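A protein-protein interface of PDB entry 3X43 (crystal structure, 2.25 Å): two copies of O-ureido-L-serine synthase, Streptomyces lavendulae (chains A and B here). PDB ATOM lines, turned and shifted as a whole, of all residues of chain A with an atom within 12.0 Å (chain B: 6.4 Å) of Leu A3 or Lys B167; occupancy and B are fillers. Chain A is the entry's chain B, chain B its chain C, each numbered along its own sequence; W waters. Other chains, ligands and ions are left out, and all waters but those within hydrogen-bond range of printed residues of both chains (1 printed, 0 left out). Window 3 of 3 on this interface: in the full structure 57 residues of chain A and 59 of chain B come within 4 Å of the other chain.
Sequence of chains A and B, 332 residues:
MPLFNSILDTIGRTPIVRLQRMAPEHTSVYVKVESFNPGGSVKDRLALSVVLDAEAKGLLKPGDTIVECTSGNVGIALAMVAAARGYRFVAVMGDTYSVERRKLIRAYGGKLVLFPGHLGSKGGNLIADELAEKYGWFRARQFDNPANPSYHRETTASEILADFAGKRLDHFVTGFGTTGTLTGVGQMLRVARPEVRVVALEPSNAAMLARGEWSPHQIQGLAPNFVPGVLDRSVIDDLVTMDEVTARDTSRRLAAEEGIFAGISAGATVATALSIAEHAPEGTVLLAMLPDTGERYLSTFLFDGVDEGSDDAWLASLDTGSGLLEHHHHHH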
ATOM      1  N   PRO A   2      26.176   4.447  -3.097  1.00  0.00           N
ATOM      2  CA  PRO A   2      25.047   4.400  -2.152  1.00  0.00           C
ATOM      3  C   PRO A   2      25.041   3.253  -1.138  1.00  0.00           C
ATOM      4  O   PRO A   2      24.376   3.349  -0.111  1.00  0.00           O
ATOM      5  CB  PRO A   2      23.782   4.442  -2.986  1.00  0.00           C
ATOM      6  CG  PRO A   2      24.236   5.318  -4.169  1.00  0.00           C
ATOM      7  CD  PRO A   2      25.782   5.180  -4.314  1.00  0.00           C
ATOM      8  N   LEU A   3      25.760   2.171  -1.415  1.00  0.00           N
ATOM      9  CA  LEU A   3      25.851   1.087  -0.437  1.00  0.00           C
ATOM     10  C   LEU A   3      26.703   1.736   0.652  1.00  0.00           C
ATOM     11  O   LEU A   3      27.639   2.461   0.332  1.00  0.00           O
ATOM     12  CB  LEU A   3      26.604  -0.099  -1.026  1.00  0.00           C
ATOM     13  CG  LEU A   3      26.079  -1.513  -0.793  1.00  0.00           C
ATOM     14  CD1 LEU A   3      24.566  -1.529  -0.847  1.00  0.00           C
ATOM     15  CD2 LEU A   3      26.662  -2.442  -1.849  1.00  0.00           C
ATOM     16  N   PHE A   4      26.388   1.522   1.925  1.00  0.00           N
ATOM     17  CA  PHE A   4      27.191   2.135   2.992  1.00  0.00           C
ATOM     18  C   PHE A   4      27.991   1.089   3.751  1.00  0.00           C
ATOM     19  O   PHE A   4      27.524  -0.025   3.994  1.00  0.00           O
ATOM     20  CB  PHE A   4      26.320   2.892   3.994  1.00  0.00           C
ATOM     21  CG  PHE A   4      25.702   4.141   3.448  1.00  0.00           C
ATOM     22  CD1 PHE A   4      24.361   4.162   3.077  1.00  0.00           C
ATOM     23  CD2 PHE A   4      26.448   5.311   3.334  1.00  0.00           C
ATOM     24  CE1 PHE A   4      23.771   5.329   2.605  1.00  0.00           C
ATOM     25  CE2 PHE A   4      25.857   6.491   2.859  1.00  0.00           C
ATOM     26  CZ  PHE A   4      24.519   6.495   2.496  1.00  0.00           C
ATOM     27  N   ASN A   5      29.201   1.465   4.137  1.00  0.00           N
ATOM     28  CA  ASN A   5      30.072   0.568   4.864  1.00  0.00           C
ATOM     29  C   ASN A   5      29.648   0.506   6.328  1.00  0.00           C
ATOM     30  O   ASN A   5      29.320  -0.558   6.848  1.00  0.00           O
ATOM     31  CB  ASN A   5      31.514   1.056   4.742  1.00  0.00           C
ATOM     32  CG  ASN A   5      32.484   0.169   5.466  1.00  0.00           C
ATOM     33  OD1 ASN A   5      32.576  -1.027   5.188  1.00  0.00           O
ATOM     34  ND2 ASN A   5      33.216   0.745   6.409  1.00  0.00           N
ATOM     35  N   SER A   6      29.641   1.660   6.983  1.00  0.00           N
ATOM     36  CA  SER A   6      29.266   1.736   8.385  1.00  0.00           C
ATOM     37  C   SER A   6      28.021   2.594   8.551  1.00  0.00           C
ATOM     38  O   SER A   6      27.781   3.510   7.762  1.00  0.00           O
ATOM     39  CB  SER A   6      30.422   2.338   9.188  1.00  0.00           C
ATOM     40  OG  SER A   6      29.977   2.928  10.397  1.00  0.00           O
ATOM     41  N   ILE A   7      27.235   2.291   9.580  1.00  0.00           N
ATOM     42  CA  ILE A   7      26.028   3.048   9.885  1.00  0.00           C
ATOM     43  C   ILE A   7      26.451   4.470  10.226  1.00  0.00           C
ATOM     44  O   ILE A   7      25.661   5.403  10.125  1.00  0.00           O
ATOM     45  CB  ILE A   7      25.301   2.473  11.101  1.00  0.00           C
ATOM     46  CG1 ILE A   7      23.985   3.219  11.335  1.00  0.00           C
ATOM     47  CG2 ILE A   7      26.180   2.617  12.335  1.00  0.00           C
ATOM     48  CD1 ILE A   7      22.908   2.892  10.321  1.00  0.00           C
ATOM     49  N   LEU A   8      27.708   4.635  10.628  1.00  0.00           N
ATOM     50  CA  LEU A   8      28.200   5.962  10.969  1.00  0.00           C
ATOM     51  C   LEU A   8      28.369   6.809   9.712  1.00  0.00           C
ATOM     52  O   LEU A   8      28.562   8.010   9.792  1.00  0.00           O
ATOM     53  CB  LEU A   8      29.534   5.868  11.719  1.00  0.00           C
ATOM     54  CG  LEU A   8      29.480   5.431  13.188  1.00  0.00           C
ATOM     55  CD1 LEU A   8      30.688   5.984  13.916  1.00  0.00           C
ATOM     56  CD2 LEU A   8      28.196   5.919  13.843  1.00  0.00           C
ATOM     57  N   ASP A   9      28.297   6.171   8.550  1.00  0.00           N
ATOM     58  CA  ASP A   9      28.427   6.881   7.280  1.00  0.00           C
ATOM     59  C   ASP A   9      27.124   7.627   6.971  1.00  0.00           C
ATOM     60  O   ASP A   9      27.079   8.495   6.099  1.00  0.00           O
ATOM     61  CB  ASP A   9      28.731   5.887   6.152  1.00  0.00           C
ATOM     62  CG  ASP A   9      30.115   5.245   6.285  1.00  0.00           C
ATOM     63  OD1 ASP A   9      30.945   5.767   7.061  1.00  0.00           O
ATOM     64  OD2 ASP A   9      30.368   4.221   5.614  1.00  0.00           O
ATOM     65  N   THR A  10      26.063   7.291   7.697  1.00  0.00           N
ATOM     66  CA  THR A  10      24.775   7.933   7.484  1.00  0.00           C
ATOM     67  C   THR A  10      24.586   9.176   8.337  1.00  0.00           C
ATOM     68  O   THR A  10      23.486   9.732   8.384  1.00  0.00           O
ATOM     69  CB  THR A  10      23.616   6.964   7.768  1.00  0.00           C
ATOM     70  OG1 THR A  10      23.607   6.603   9.157  1.00  0.00           O
ATOM     71  CG2 THR A  10      23.754   5.726   6.916  1.00  0.00           C
ATOM     72  N   ILE A  11      25.654   9.625   8.998  1.00  0.00           N
ATOM     73  CA  ILE A  11      25.559  10.804   9.858  1.00  0.00           C
ATOM     74  C   ILE A  11      25.621  12.118   9.075  1.00  0.00           C
ATOM     75  O   ILE A  11      26.459  12.295   8.187  1.00  0.00           O
ATOM     76  CB  ILE A  11      26.664  10.785  10.946  1.00  0.00           C
ATOM     77  CG1 ILE A  11      26.385   9.648  11.942  1.00  0.00           C
ATOM     78  CG2 ILE A  11      26.698  12.119  11.695  1.00  0.00           C
ATOM     79  CD1 ILE A  11      27.513   9.402  12.958  1.00  0.00           C
ATOM     80  N   ARG A  13      23.961  15.352   6.641  1.00  0.00           N
ATOM     81  CA  ARG A  13      23.204  15.479   5.400  1.00  0.00           C
ATOM     82  C   ARG A  13      21.708  15.338   5.693  1.00  0.00           C
ATOM     83  O   ARG A  13      20.969  14.669   4.976  1.00  0.00           O
ATOM     84  CB  ARG A  13      23.645  14.422   4.385  1.00  0.00           C
ATOM     85  CG  ARG A  13      25.074  14.598   3.862  1.00  0.00           C
ATOM     86  CD  ARG A  13      25.392  13.553   2.800  1.00  0.00           C
ATOM     87  NE  ARG A  13      25.170  12.204   3.316  1.00  0.00           N
ATOM     88  CZ  ARG A  13      26.005  11.566   4.136  1.00  0.00           C
ATOM     89  NH1 ARG A  13      27.133  12.146   4.539  1.00  0.00           N
ATOM     90  NH2 ARG A  13      25.686  10.366   4.597  1.00  0.00           N
ATOM     91  N   ILE B  16      21.347   1.203   3.181  1.00  0.00           N
ATOM     92  CA  ILE B  16      21.697  -0.200   3.315  1.00  0.00           C
ATOM     93  C   ILE B  16      23.160  -0.142   3.798  1.00  0.00           C
ATOM     94  O   ILE B  16      24.023   0.429   3.117  1.00  0.00           O
ATOM     95  CB  ILE B  16      21.591  -0.926   1.952  1.00  0.00           C
ATOM     96  CG1 ILE B  16      20.125  -1.002   1.514  1.00  0.00           C
ATOM     97  CG2 ILE B  16      22.178  -2.321   2.045  1.00  0.00           C
ATOM     98  CD1 ILE B  16      19.908  -1.713   0.140  1.00  0.00           C
ATOM     99  N   VAL B  17      23.420  -0.669   4.997  1.00  0.00           N
ATOM    100  CA  VAL B  17      24.771  -0.678   5.554  1.00  0.00           C
ATOM    101  C   VAL B  17      25.263  -2.110   5.796  1.00  0.00           C
ATOM    102  O   VAL B  17      24.473  -3.021   6.030  1.00  0.00           O
ATOM    103  CB  VAL B  17      24.854   0.100   6.910  1.00  0.00           C
ATOM    104  CG1 VAL B  17      23.907   1.297   6.906  1.00  0.00           C
ATOM    105  CG2 VAL B  17      24.506  -0.824   8.065  1.00  0.00           C
ATOM    106  N   TYR B  30      24.361  -7.438   4.669  1.00  0.00           N
ATOM    107  CA  TYR B  30      23.925  -6.055   4.551  1.00  0.00           C
ATOM    108  C   TYR B  30      22.574  -5.854   5.207  1.00  0.00           C
ATOM    109  O   TYR B  30      21.737  -6.759   5.254  1.00  0.00           O
ATOM    110  CB  TYR B  30      23.858  -5.663   3.075  1.00  0.00           C
ATOM    111  CG  TYR B  30      25.212  -5.333   2.494  1.00  0.00           C
ATOM    112  CD1 TYR B  30      25.890  -6.241   1.681  1.00  0.00           C
ATOM    113  CD2 TYR B  30      25.816  -4.113   2.767  1.00  0.00           C
ATOM    114  CE1 TYR B  30      27.150  -5.927   1.155  1.00  0.00           C
ATOM    115  CE2 TYR B  30      27.060  -3.802   2.251  1.00  0.00           C
ATOM    116  CZ  TYR B  30      27.720  -4.705   1.449  1.00  0.00           C
ATOM    117  OH  TYR B  30      28.956  -4.364   0.953  1.00  0.00           O
ATOM    118  N   ILE B 160      17.088  -1.131  -3.403  1.00  0.00           N
ATOM    119  CA  ILE B 160      17.869  -2.359  -3.271  1.00  0.00           C
ATOM    120  C   ILE B 160      18.560  -2.702  -4.600  1.00  0.00           C
ATOM    121  O   ILE B 160      19.751  -2.969  -4.630  1.00  0.00           O
ATOM    122  CB  ILE B 160      16.959  -3.517  -2.827  1.00  0.00           C
ATOM    123  CG1 ILE B 160      16.412  -3.223  -1.422  1.00  0.00           C
ATOM    124  CG2 ILE B 160      17.714  -4.840  -2.880  1.00  0.00           C
ATOM    125  CD1 ILE B 160      15.478  -4.311  -0.862  1.00  0.00           C
ATOM    126  N   ASP B 163      21.431  -0.110  -5.408  1.00  0.00           N
ATOM    127  CA  ASP B 163      22.602  -0.232  -4.533  1.00  0.00           C
ATOM    128  C   ASP B 163      23.430  -1.476  -4.860  1.00  0.00           C
ATOM    129  O   ASP B 163      24.642  -1.490  -4.670  1.00  0.00           O
ATOM    130  CB  ASP B 163      22.178  -0.311  -3.060  1.00  0.00           C
ATOM    131  CG  ASP B 163      21.806   1.040  -2.479  1.00  0.00           C
ATOM    132  OD1 ASP B 163      21.846   2.045  -3.212  1.00  0.00           O
ATOM    133  OD2 ASP B 163      21.465   1.099  -1.282  1.00  0.00           O
ATOM    134  N   PHE B 164      22.772  -2.519  -5.354  1.00  0.00           N
ATOM    135  CA  PHE B 164      23.467  -3.753  -5.665  1.00  0.00           C
ATOM    136  C   PHE B 164      23.758  -3.965  -7.146  1.00  0.00           C
ATOM    137  O   PHE B 164      24.349  -4.973  -7.522  1.00  0.00           O
ATOM    138  CB  PHE B 164      22.676  -4.935  -5.094  1.00  0.00           C
ATOM    139  CG  PHE B 164      22.901  -5.136  -3.622  1.00  0.00           C
ATOM    140  CD1 PHE B 164      21.970  -4.686  -2.691  1.00  0.00           C
ATOM    141  CD2 PHE B 164      24.080  -5.731  -3.160  1.00  0.00           C
ATOM    142  CE1 PHE B 164      22.206  -4.816  -1.327  1.00  0.00           C
ATOM    143  CE2 PHE B 164      24.323  -5.869  -1.795  1.00  0.00           C
ATOM    144  CZ  PHE B 164      23.383  -5.407  -0.877  1.00  0.00           C
ATOM    145  N   ALA B 165      23.352  -3.018  -7.986  1.00  0.00           N
ATOM    146  CA  ALA B 165      23.585  -3.130  -9.425  1.00  0.00           C
ATOM    147  C   ALA B 165      25.061  -3.417  -9.749  1.00  0.00           C
ATOM    148  O   ALA B 165      25.961  -2.701  -9.306  1.00  0.00           O
ATOM    149  CB  ALA B 165      23.132  -1.854 -10.129  1.00  0.00           C
ATOM    150  N   GLY B 166      25.297  -4.473 -10.522  1.00  0.00           N
ATOM    151  CA  GLY B 166      26.658  -4.830 -10.887  1.00  0.00           C
ATOM    152  C   GLY B 166      27.472  -5.331  -9.704  1.00  0.00           C
ATOM    153  O   GLY B 166      28.709  -5.345  -9.740  1.00  0.00           O
ATOM    154  N   LYS B 167      26.777  -5.735  -8.647  1.00  0.00           N
ATOM    155  CA  LYS B 167      27.434  -6.236  -7.449  1.00  0.00           C
ATOM    156  C   LYS B 167      26.769  -7.558  -7.086  1.00  0.00           C
ATOM    157  O   LYS B 167      25.659  -7.835  -7.528  1.00  0.00           O
ATOM    158  CB  LYS B 167      27.275  -5.241  -6.297  1.00  0.00           C
ATOM    159  CG  LYS B 167      28.262  -4.094  -6.297  1.00  0.00           C
ATOM    160  CD  LYS B 167      27.942  -3.124  -5.165  1.00  0.00           C
ATOM    161  CE  LYS B 167      29.043  -2.104  -4.957  1.00  0.00           C
ATOM    162  NZ  LYS B 167      29.254  -1.243  -6.150  1.00  0.00           N
ATOM    163  N   ARG B 168      27.435  -8.368  -6.270  1.00  0.00           N
ATOM    164  CA  ARG B 168      26.883  -9.659  -5.878  1.00  0.00           C
ATOM    165  C   ARG B 168      25.797  -9.568  -4.808  1.00  0.00           C
ATOM    166  O   ARG B 168      25.905  -8.795  -3.864  1.00  0.00           O
ATOM    167  CB  ARG B 168      28.010 -10.573  -5.386  1.00  0.00           C
ATOM    168  CG  ARG B 168      27.627 -12.044  -5.324  1.00  0.00           C
ATOM    169  CD  ARG B 168      28.708 -12.862  -4.629  1.00  0.00           C
ATOM    170  NE  ARG B 168      28.194 -14.121  -4.091  1.00  0.00           N
ATOM    171  CZ  ARG B 168      28.882 -15.260  -4.087  1.00  0.00           C
ATOM    172  NH1 ARG B 168      30.106 -15.294  -4.592  1.00  0.00           N
ATOM    173  NH2 ARG B 168      28.351 -16.359  -3.570  1.00  0.00           N
ATOM    174  N   LEU B 169      24.754 -10.374  -4.968  1.00  0.00           N
ATOM    175  CA  LEU B 169      23.640 -10.436  -4.023  1.00  0.00           C
ATOM    176  C   LEU B 169      23.006 -11.823  -4.135  1.00  0.00           C
ATOM    177  O   LEU B 169      22.481 -12.191  -5.192  1.00  0.00           O
ATOM    178  CB  LEU B 169      22.588  -9.355  -4.336  1.00  0.00           C
ATOM    179  CG  LEU B 169      21.349  -9.356  -3.429  1.00  0.00           C
ATOM    180  CD1 LEU B 169      21.772  -9.399  -1.965  1.00  0.00           C
ATOM    181  CD2 LEU B 169      20.517  -8.124  -3.696  1.00  0.00           C
ATOM    182  N   ARG B 193      16.751  -9.975 -10.638  1.00  0.00           N
ATOM    183  CA  ARG B 193      17.806 -10.841 -10.119  1.00  0.00           C
ATOM    184  C   ARG B 193      17.198 -12.171  -9.695  1.00  0.00           C
ATOM    185  O   ARG B 193      17.076 -12.461  -8.507  1.00  0.00           O
ATOM    186  CB  ARG B 193      18.487 -10.194  -8.915  1.00  0.00           C
ATOM    187  CG  ARG B 193      18.959  -8.773  -9.144  1.00  0.00           C
ATOM    188  CD  ARG B 193      20.387  -8.766  -9.602  1.00  0.00           C
ATOM    189  NE  ARG B 193      21.291  -8.158  -8.635  1.00  0.00           N
ATOM    190  CZ  ARG B 193      22.357  -8.771  -8.132  1.00  0.00           C
ATOM    191  NH1 ARG B 193      22.646 -10.002  -8.502  1.00  0.00           N
ATOM    192  NH2 ARG B 193      23.157  -8.138  -7.288  1.00  0.00           N
HETATM  193  O   HOH W   1      21.965   2.797   0.675  1.00  0.00           O
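Among the printed residues, merely in contact across the chains: Pro A2 with Asp B163 (3.1 Å), Leu A3 with Ile B16 (3.8 Å), Leu A3 with Tyr B30 (3.9 Å), Leu A3 with Asp B163 (3.5 Å), Leu A3 with Lys B167 (3.6 Å), Phe A4 with Val B17 (3.2 Å) and Ile A7 with Val B17 (3.9 Å).
The guanidinium group (NH2) of Arg B193 is in hydrogen-bond range of the backbone carbonyl oxygen (O) of Lys B167 (2.5 Å). O of Ile A7 is in hydrogen-bond range of OG1 of Thr A10 (2.6 Å).
Hydrophobic or aromatic side chains of chain B that line the printed part of chain A: Ile B16, Val B17 and Tyr B30. Among the printed residues, 8 pairs touch across the chains.
No position is printed for both chains.
O of Ile B16 lies within hydrogen-bond range of N of Phe A4, 2.9 Å away.
Water W1 lies within hydrogen-bond range of the backbone carbonyl oxygen of Pro A2 (2.6 Å), the side-chain carboxylate of Asp B163 (2.6 Å) and the backbone NH of Ile B16 (3.0 Å).
Printed residues of chain B within 4 Å of Pro A2: Asp B163. Printed residues of chain B within 4 Å of Phe A4: Ile B16 and Val B17. Of the printed residues of chain B, Ile A7 touches Val B17 (3.9 Å). Thr A10 touches none of the printed residues of chain B. Ile A11 touches none of the printed residues of chain B. Of chain A, only Leu A3 (3.8 Å) and Phe A4 (2.9 Å) come within 4 Å of Ile B16. Printed residues of chain A within 4 Å of Val B17: Phe A4 and Ile A7. Asp B163 touches just these residues of chain A: Pro A2 and Leu A3. No residue of chain A comes within 4 Å of Ala B165. Lys B167 touches just one residue of chain A: Leu A3. The nearest residue of chain B that does not touch Leu A3 is Phe B164 (4.1 Å). The nearest residue of chain A that does not touch Lys B167 is Pro A2 (7.2 Å). The nearest printed residue of chain B that does not touch Ile A7 is Ile B16 (7.2 Å).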
